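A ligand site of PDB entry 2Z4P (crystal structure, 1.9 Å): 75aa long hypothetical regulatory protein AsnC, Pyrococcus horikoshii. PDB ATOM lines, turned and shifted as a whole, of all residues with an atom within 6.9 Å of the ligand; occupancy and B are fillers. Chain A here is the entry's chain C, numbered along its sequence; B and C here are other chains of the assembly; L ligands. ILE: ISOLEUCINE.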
ATOM      1  N   THR A  10      29.582  29.856 -29.137  1.00  0.00           N
ATOM      2  CA  THR A  10      30.547  30.356 -28.165  1.00  0.00           C
ATOM      3  C   THR A  10      30.745  29.309 -27.079  1.00  0.00           C
ATOM      4  O   THR A  10      29.988  28.330 -26.992  1.00  0.00           O
ATOM      5  CB  THR A  10      30.053  31.626 -27.457  1.00  0.00           C
ATOM      6  OG1 THR A  10      28.970  31.290 -26.578  1.00  0.00           O
ATOM      7  CG2 THR A  10      29.564  32.649 -28.486  1.00  0.00           C
ATOM      8  N   GLU A  15      28.467  33.566 -24.034  1.00  0.00           N
ATOM      9  CA  GLU A  15      27.780  34.283 -25.113  1.00  0.00           C
ATOM     10  C   GLU A  15      27.449  35.753 -24.856  1.00  0.00           C
ATOM     11  O   GLU A  15      27.621  36.580 -25.756  1.00  0.00           O
ATOM     12  CB  GLU A  15      26.511  33.529 -25.553  1.00  0.00           C
ATOM     13  CG  GLU A  15      25.439  33.313 -24.489  1.00  0.00           C
ATOM     14  CD  GLU A  15      25.615  32.011 -23.701  1.00  0.00           C
ATOM     15  OE1 GLU A  15      24.621  31.590 -23.067  1.00  0.00           O
ATOM     16  OE2 GLU A  15      26.728  31.424 -23.698  1.00  0.00           O
ATOM     17  N   VAL A  33      21.632  36.994 -28.598  1.00  0.00           N
ATOM     18  CA  VAL A  33      21.921  35.644 -28.122  1.00  0.00           C
ATOM     19  C   VAL A  33      20.666  34.890 -28.598  1.00  0.00           C
ATOM     20  O   VAL A  33      19.547  35.374 -28.419  1.00  0.00           O
ATOM     21  CB  VAL A  33      21.988  35.565 -26.573  1.00  0.00           C
ATOM     22  CG1 VAL A  33      21.997  34.103 -26.137  1.00  0.00           C
ATOM     23  CG2 VAL A  33      23.249  36.268 -26.071  1.00  0.00           C
ATOM     24  N   VAL A  34      20.844  33.728 -29.215  1.00  0.00           N
ATOM     25  CA  VAL A  34      19.717  32.966 -29.735  1.00  0.00           C
ATOM     26  C   VAL A  34      19.687  31.490 -29.341  1.00  0.00           C
ATOM     27  O   VAL A  34      20.707  30.917 -28.964  1.00  0.00           O
ATOM     28  CB  VAL A  34      19.679  33.025 -31.274  1.00  0.00           C
ATOM     29  CG1 VAL A  34      19.493  34.460 -31.763  1.00  0.00           C
ATOM     30  CG2 VAL A  34      20.961  32.429 -31.826  1.00  0.00           C
ATOM     31  N   TYR A  35      18.493  30.900 -29.427  1.00  0.00           N
ATOM     32  CA  TYR A  35      18.269  29.477 -29.144  1.00  0.00           C
ATOM     33  C   TYR A  35      18.598  28.656 -30.379  1.00  0.00           C
ATOM     34  O   TYR A  35      18.382  29.098 -31.511  1.00  0.00           O
ATOM     35  CB  TYR A  35      16.809  29.225 -28.779  1.00  0.00           C
ATOM     36  CG  TYR A  35      16.450  29.642 -27.378  1.00  0.00           C
ATOM     37  CD1 TYR A  35      16.624  28.757 -26.311  1.00  0.00           C
ATOM     38  CD2 TYR A  35      15.929  30.916 -27.106  1.00  0.00           C
ATOM     39  CE1 TYR A  35      16.286  29.126 -25.011  1.00  0.00           C
ATOM     40  CE2 TYR A  35      15.589  31.286 -25.792  1.00  0.00           C
ATOM     41  CZ  TYR A  35      15.765  30.373 -24.750  1.00  0.00           C
ATOM     42  OH  TYR A  35      15.421  30.696 -23.452  1.00  0.00           O
ATOM     43  N   GLY A  36      19.108  27.458 -30.169  1.00  0.00           N
ATOM     44  CA  GLY A  36      19.417  26.599 -31.300  1.00  0.00           C
ATOM     45  C   GLY A  36      20.871  26.162 -31.324  1.00  0.00           C
ATOM     46  O   GLY A  36      21.589  26.299 -30.327  1.00  0.00           O
ATOM     47  N   GLU A  37      21.287  25.632 -32.461  1.00  0.00           N
ATOM     48  CA  GLU A  37      22.654  25.167 -32.655  1.00  0.00           C
ATOM     49  C   GLU A  37      23.644  26.328 -32.456  1.00  0.00           C
ATOM     50  O   GLU A  37      24.732  26.138 -31.928  1.00  0.00           O
ATOM     51  CB  GLU A  37      22.790  24.611 -34.083  1.00  0.00           C
ATOM     52  CG  GLU A  37      24.152  24.050 -34.444  1.00  0.00           C
ATOM     53  CD  GLU A  37      24.288  23.831 -35.939  1.00  0.00           C
ATOM     54  OE1 GLU A  37      23.301  23.390 -36.569  1.00  0.00           O
ATOM     55  OE2 GLU A  37      25.384  24.102 -36.489  1.00  0.00           O
ATOM     56  N   TYR A  38      23.250  27.521 -32.896  1.00  0.00           N
ATOM     57  CA  TYR A  38      24.092  28.696 -32.752  1.00  0.00           C
ATOM     58  C   TYR A  38      23.716  29.442 -31.489  1.00  0.00           C
ATOM     59  O   TYR A  38      22.593  29.320 -31.000  1.00  0.00           O
ATOM     60  CB  TYR A  38      23.927  29.608 -33.972  1.00  0.00           C
ATOM     61  CG  TYR A  38      24.452  28.990 -35.238  1.00  0.00           C
ATOM     62  CD1 TYR A  38      25.822  28.806 -35.421  1.00  0.00           C
ATOM     63  CD2 TYR A  38      23.586  28.565 -36.236  1.00  0.00           C
ATOM     64  CE1 TYR A  38      26.314  28.208 -36.576  1.00  0.00           C
ATOM     65  CE2 TYR A  38      24.066  27.962 -37.398  1.00  0.00           C
ATOM     66  CZ  TYR A  38      25.430  27.785 -37.561  1.00  0.00           C
ATOM     67  OH  TYR A  38      25.910  27.185 -38.695  1.00  0.00           O
ATOM     68  N   ASP A  39      24.652  30.217 -30.956  1.00  0.00           N
ATOM     69  CA  ASP A  39      24.411  30.951 -29.730  1.00  0.00           C
ATOM     70  C   ASP A  39      24.256  32.452 -29.927  1.00  0.00           C
ATOM     71  O   ASP A  39      23.669  33.138 -29.084  1.00  0.00           O
ATOM     72  CB  ASP A  39      25.560  30.686 -28.743  1.00  0.00           C
ATOM     73  CG  ASP A  39      25.790  29.207 -28.525  1.00  0.00           C
ATOM     74  OD1 ASP A  39      24.788  28.458 -28.466  1.00  0.00           O
ATOM     75  OD2 ASP A  39      26.979  28.799 -28.397  1.00  0.00           O
ATOM     76  N   LEU A  40      24.796  32.953 -31.034  1.00  0.00           N
ATOM     77  CA  LEU A  40      24.738  34.374 -31.361  1.00  0.00           C
ATOM     78  C   LEU A  40      24.541  34.612 -32.840  1.00  0.00           C
ATOM     79  O   LEU A  40      25.024  33.829 -33.675  1.00  0.00           O
ATOM     80  CB  LEU A  40      26.049  35.081 -30.971  1.00  0.00           C
ATOM     81  CG  LEU A  40      26.487  35.223 -29.520  1.00  0.00           C
ATOM     82  CD1 LEU A  40      27.879  35.841 -29.488  1.00  0.00           C
ATOM     83  CD2 LEU A  40      25.514  36.087 -28.753  1.00  0.00           C
ATOM     84  N   ILE B   6      16.491  20.340 -24.306  1.00  0.00           N
ATOM     85  CA  ILE B   6      17.872  20.756 -24.415  1.00  0.00           C
ATOM     86  C   ILE B   6      18.715  19.563 -24.821  1.00  0.00           C
ATOM     87  O   ILE B   6      18.695  18.521 -24.148  1.00  0.00           O
ATOM     88  CB  ILE B   6      18.461  21.248 -23.070  1.00  0.00           C
ATOM     89  CG1 ILE B   6      17.572  22.299 -22.428  1.00  0.00           C
ATOM     90  CG2 ILE B   6      19.857  21.812 -23.323  1.00  0.00           C
ATOM     91  CD1 ILE B   6      17.992  22.647 -21.009  1.00  0.00           C
ATOM     92  N   LEU B   7      19.453  19.716 -25.918  1.00  0.00           N
ATOM     93  CA  LEU B   7      20.366  18.676 -26.390  1.00  0.00           C
ATOM     94  C   LEU B   7      21.720  19.156 -25.866  1.00  0.00           C
ATOM     95  O   LEU B   7      22.119  20.298 -26.132  1.00  0.00           O
ATOM     96  CB  LEU B   7      20.369  18.633 -27.923  1.00  0.00           C
ATOM     97  CG  LEU B   7      19.011  18.412 -28.597  1.00  0.00           C
ATOM     98  CD1 LEU B   7      19.175  18.441 -30.112  1.00  0.00           C
ATOM     99  CD2 LEU B   7      18.406  17.077 -28.131  1.00  0.00           C
ATOM    100  N   LEU B  52      12.727  30.835 -18.885  1.00  0.00           N
ATOM    101  CA  LEU B  52      13.548  29.861 -19.602  1.00  0.00           C
ATOM    102  C   LEU B  52      14.850  30.551 -20.008  1.00  0.00           C
ATOM    103  O   LEU B  52      15.935  29.987 -19.844  1.00  0.00           O
ATOM    104  CB  LEU B  52      12.829  29.347 -20.849  1.00  0.00           C
ATOM    105  CG  LEU B  52      13.666  28.353 -21.663  1.00  0.00           C
ATOM    106  CD1 LEU B  52      13.760  27.048 -20.857  1.00  0.00           C
ATOM    107  CD2 LEU B  52      13.007  28.093 -23.029  1.00  0.00           C
ATOM    108  N   ASP B  53      14.748  31.776 -20.542  1.00  0.00           N
ATOM    109  CA  ASP B  53      15.945  32.516 -20.943  1.00  0.00           C
ATOM    110  C   ASP B  53      16.948  32.541 -19.781  1.00  0.00           C
ATOM    111  O   ASP B  53      18.134  32.254 -19.965  1.00  0.00           O
ATOM    112  CB  ASP B  53      15.628  33.969 -21.303  1.00  0.00           C
ATOM    113  CG  ASP B  53      14.807  34.113 -22.578  1.00  0.00           C
ATOM    114  OD1 ASP B  53      14.706  33.157 -23.363  1.00  0.00           O
ATOM    115  OD2 ASP B  53      14.274  35.216 -22.799  1.00  0.00           O
ATOM    116  N   ILE B  56      18.395  28.897 -18.850  1.00  0.00           N
ATOM    117  CA  ILE B  56      19.399  28.391 -19.763  1.00  0.00           C
ATOM    118  C   ILE B  56      20.714  29.161 -19.715  1.00  0.00           C
ATOM    119  O   ILE B  56      21.779  28.566 -19.641  1.00  0.00           O
ATOM    120  CB  ILE B  56      18.897  28.367 -21.222  1.00  0.00           C
ATOM    121  CG1 ILE B  56      17.618  27.528 -21.326  1.00  0.00           C
ATOM    122  CG2 ILE B  56      19.970  27.775 -22.131  1.00  0.00           C
ATOM    123  CD1 ILE B  56      17.802  26.083 -20.956  1.00  0.00           C
ATOM    124  N   THR B  57      20.642  30.496 -19.755  1.00  0.00           N
ATOM    125  CA  THR B  57      21.861  31.294 -19.756  1.00  0.00           C
ATOM    126  C   THR B  57      22.579  31.449 -18.411  1.00  0.00           C
ATOM    127  O   THR B  57      23.803  31.426 -18.368  1.00  0.00           O
ATOM    128  CB  THR B  57      21.619  32.714 -20.302  1.00  0.00           C
ATOM    129  OG1 THR B  57      20.640  33.378 -19.484  1.00  0.00           O
ATOM    130  CG2 THR B  57      21.123  32.662 -21.751  1.00  0.00           C
ATOM    131  N   ILE B  60      22.017  26.648 -16.496  1.00  0.00           N
ATOM    132  CA  ILE B  60      22.525  25.578 -17.326  1.00  0.00           C
ATOM    133  C   ILE B  60      23.867  25.824 -17.987  1.00  0.00           C
ATOM    134  O   ILE B  60      24.804  25.046 -17.818  1.00  0.00           O
ATOM    135  CB  ILE B  60      21.507  25.189 -18.433  1.00  0.00           C
ATOM    136  CG1 ILE B  60      20.185  24.717 -17.804  1.00  0.00           C
ATOM    137  CG2 ILE B  60      22.091  24.087 -19.293  1.00  0.00           C
ATOM    138  CD1 ILE B  60      20.310  23.458 -16.923  1.00  0.00           C
ATOM    139  N   ARG B  61      23.988  26.896 -18.759  1.00  0.00           N
ATOM    140  CA  ARG B  61      25.245  27.126 -19.456  1.00  0.00           C
ATOM    141  C   ARG B  61      26.421  27.591 -18.588  1.00  0.00           C
ATOM    142  O   ARG B  61      27.539  27.728 -19.079  1.00  0.00           O
ATOM    143  CB  ARG B  61      25.004  28.070 -20.647  1.00  0.00           C
ATOM    144  CG  ARG B  61      24.237  27.343 -21.778  1.00  0.00           C
ATOM    145  CD  ARG B  61      23.892  28.252 -22.947  1.00  0.00           C
ATOM    146  NE  ARG B  61      25.065  28.786 -23.638  1.00  0.00           N
ATOM    147  CZ  ARG B  61      25.685  28.197 -24.647  1.00  0.00           C
ATOM    148  NH1 ARG B  61      25.264  27.017 -25.111  1.00  0.00           N
ATOM    149  NH2 ARG B  61      26.716  28.805 -25.231  1.00  0.00           N
ATOM    150  N   MET B  68      28.297  22.288 -24.532  1.00  0.00           N
ATOM    151  CA  MET B  68      27.407  22.808 -25.560  1.00  0.00           C
ATOM    152  C   MET B  68      25.945  22.501 -25.281  1.00  0.00           C
ATOM    153  O   MET B  68      25.628  21.479 -24.684  1.00  0.00           O
ATOM    154  CB  MET B  68      27.739  22.206 -26.926  1.00  0.00           C
ATOM    155  CG  MET B  68      29.026  22.690 -27.565  1.00  0.00           C
ATOM    156  SD  MET B  68      29.336  21.804 -29.114  1.00  0.00           S
ATOM    157  CE  MET B  68      30.779  20.794 -28.653  1.00  0.00           C
ATOM    158  N   THR B  69      25.068  23.399 -25.704  1.00  0.00           N
ATOM    159  CA  THR B  69      23.638  23.180 -25.555  1.00  0.00           C
ATOM    160  C   THR B  69      22.934  23.724 -26.786  1.00  0.00           C
ATOM    161  O   THR B  69      23.330  24.758 -27.318  1.00  0.00           O
ATOM    162  CB  THR B  69      23.016  23.877 -24.316  1.00  0.00           C
ATOM    163  OG1 THR B  69      23.124  25.309 -24.446  1.00  0.00           O
ATOM    164  CG2 THR B  69      23.689  23.410 -23.030  1.00  0.00           C
ATOM    165  N   SER B  70      21.925  22.995 -27.235  1.00  0.00           N
ATOM    166  CA  SER B  70      21.104  23.409 -28.370  1.00  0.00           C
ATOM    167  C   SER B  70      19.690  23.177 -27.834  1.00  0.00           C
ATOM    168  O   SER B  70      19.249  22.044 -27.663  1.00  0.00           O
ATOM    169  CB  SER B  70      21.386  22.524 -29.584  1.00  0.00           C
ATOM    170  OG  SER B  70      20.569  22.903 -30.672  1.00  0.00           O
ATOM    171  N   THR B  71      18.985  24.276 -27.541  1.00  0.00           N
ATOM    172  CA  THR B  71      17.656  24.196 -26.963  1.00  0.00           C
ATOM    173  C   THR B  71      16.538  24.362 -28.001  1.00  0.00           C
ATOM    174  O   THR B  71      16.527  25.330 -28.773  1.00  0.00           O
ATOM    175  CB  THR B  71      17.519  25.241 -25.826  1.00  0.00           C
ATOM    176  OG1 THR B  71      18.559  25.014 -24.861  1.00  0.00           O
ATOM    177  CG2 THR B  71      16.164  25.142 -25.133  1.00  0.00           C
ATOM    178  N   MET B  72      15.610  23.409 -28.001  1.00  0.00           N
ATOM    179  CA  MET B  72      14.490  23.413 -28.936  1.00  0.00           C
ATOM    180  C   MET B  72      13.193  23.707 -28.186  1.00  0.00           C
ATOM    181  O   MET B  72      12.651  22.853 -27.473  1.00  0.00           O
ATOM    182  CB  MET B  72      14.378  22.044 -29.624  1.00  0.00           C
ATOM    183  CG  MET B  72      15.670  21.681 -30.374  1.00  0.00           C
ATOM    184  SD  MET B  72      15.590  20.040 -31.108  1.00  0.00           S
ATOM    185  CE  MET B  72      15.846  19.035 -29.655  1.00  0.00           C
ATOM    186  N   ILE C  73      14.911  31.767 -31.985  1.00  0.00           N
ATOM    187  CA  ILE C  73      14.331  32.736 -31.067  1.00  0.00           C
ATOM    188  C   ILE C  73      15.446  33.466 -30.316  1.00  0.00           C
ATOM    189  O   ILE C  73      16.425  32.840 -29.893  1.00  0.00           O
ATOM    190  CB  ILE C  73      13.381  32.010 -30.083  1.00  0.00           C
ATOM    191  CG1 ILE C  73      12.132  31.568 -30.850  1.00  0.00           C
ATOM    192  CG2 ILE C  73      13.037  32.910 -28.908  1.00  0.00           C
ATOM    193  CD1 ILE C  73      11.268  30.574 -30.132  1.00  0.00           C
ATOM    194  N   ILE C  75      17.030  36.020 -27.172  1.00  0.00           N
ATOM    195  CA  ILE C  75      16.827  36.339 -25.769  1.00  0.00           C
ATOM    196  C   ILE C  75      16.669  37.854 -25.697  1.00  0.00           C
ATOM    197  O   ILE C  75      17.320  38.547 -26.531  1.00  0.00           O
ATOM    198  CB  ILE C  75      18.050  35.925 -24.899  1.00  0.00           C
ATOM    199  CG1 ILE C  75      18.048  34.414 -24.671  1.00  0.00           C
ATOM    200  CG2 ILE C  75      18.002  36.644 -23.558  1.00  0.00           C
ATOM    201  CD1 ILE C  75      18.291  33.592 -25.908  1.00  0.00           C
ATOM    202  OXT ILE C  75      15.915  38.340 -24.830  1.00  0.00           O
HETATM  203  N   ILE L   1      21.907  28.417 -28.299  1.00  0.00           N
HETATM  204  CA  ILE L   1      21.923  27.919 -26.890  1.00  0.00           C
HETATM  205  C   ILE L   1      20.809  26.910 -26.662  1.00  0.00           C
HETATM  206  O   ILE L   1      19.895  26.838 -27.517  1.00  0.00           O
HETATM  207  CB  ILE L   1      21.755  29.073 -25.880  1.00  0.00           C
HETATM  208  CG1 ILE L   1      20.381  29.707 -26.039  1.00  0.00           C
HETATM  209  CG2 ILE L   1      22.834  30.122 -26.091  1.00  0.00           C
HETATM  210  CD1 ILE L   1      20.079  30.762 -24.987  1.00  0.00           C
HETATM  211  OXT ILE L   1      20.851  26.201 -25.633  1.00  0.00           O
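The side-chain carboxylate (OD1) of Asp 39 is in salt-bridge range of a nitrogen (N) of the ligand, at 2.9 Å. The backbone carbonyl oxygen (O) of Gly 36 lies within hydrogen-bond range of a nitrogen (N) of the ligand (2.9 Å). N of Gly 36 is in hydrogen-bond range of O of the ligand, 2.8 Å away. The backbone carbonyl oxygen (O) of Val 34 is in hydrogen-bond range of a nitrogen (N) of the ligand (2.9 Å). The backbone carbonyl oxygen of Tyr 38 sits at hydrogen-bond distance from a nitrogen (N) of the ligand, 2.9 Å away. An oxygen (O) of the ligand lies within hydrogen-bond range of the backbone NH of Thr 71 of chain B (2.7 Å). The side-chain hydroxyl (OG1) of Thr 69 of chain B sits at hydrogen-bond distance from an oxygen (OXT) of the ligand, 2.7 Å away. OG1 of Thr 71 of chain B sits at hydrogen-bond distance from OXT of the ligand (2.7 Å).
Residues that only touch the ligand: Glu 15, Tyr 35, Ile 56 of chain B, Thr 57 of chain B, Arg 61 of chain B, Ser 70 of chain B and Ile 75 of chain C. Hydrophobic or aromatic side chains that line the ligand: Tyr 35, Ile 56 of chain B and Ile 75 of chain C. Within 4 Å of the ligand: Glu 15, Val 34, Tyr 35, Gly 36, Tyr 38, Asp 39, Ile 56 of chain B, Thr 57 of chain B, Arg 61 of chain B, Thr 69 of chain B, Ser 70 of chain B, Thr 71 of chain B and Ile 75 of chain C. The nearest printed residue that does not touch the ligand is Val 33 (4.02 Å).
OD2 of Asp 39 is in salt-bridge range of NH2 of Arg 61 of chain B, at 3.2 Å. OD1 of Asp 53 of chain B sits at hydrogen-bond distance from OH of Tyr 35 (2.6 Å). N of Leu 7 of chain B sits at hydrogen-bond distance from O of Ser 70 of chain B (2.9 Å). The backbone carbonyl oxygen of Val 33 sits at hydrogen-bond distance from the backbone NH of Ile 75 of chain C (2.9 Å). The backbone NH (N) of Glu 37 is in hydrogen-bond range of the side-chain hydroxyl (OG) of Ser 70 of chain B, at 3.3 Å. The backbone NH of Glu 15 sits at hydrogen-bond distance from the side-chain hydroxyl of Thr 10. The backbone carbonyl oxygen (O) of Ile 73 of chain C sits at hydrogen-bond distance from the backbone NH (N) of Tyr 35 (2.9 Å). The backbone NH of Arg 61 of chain B sits at hydrogen-bond distance from the backbone carbonyl oxygen of Ile 56 of chain B (2.9 Å).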
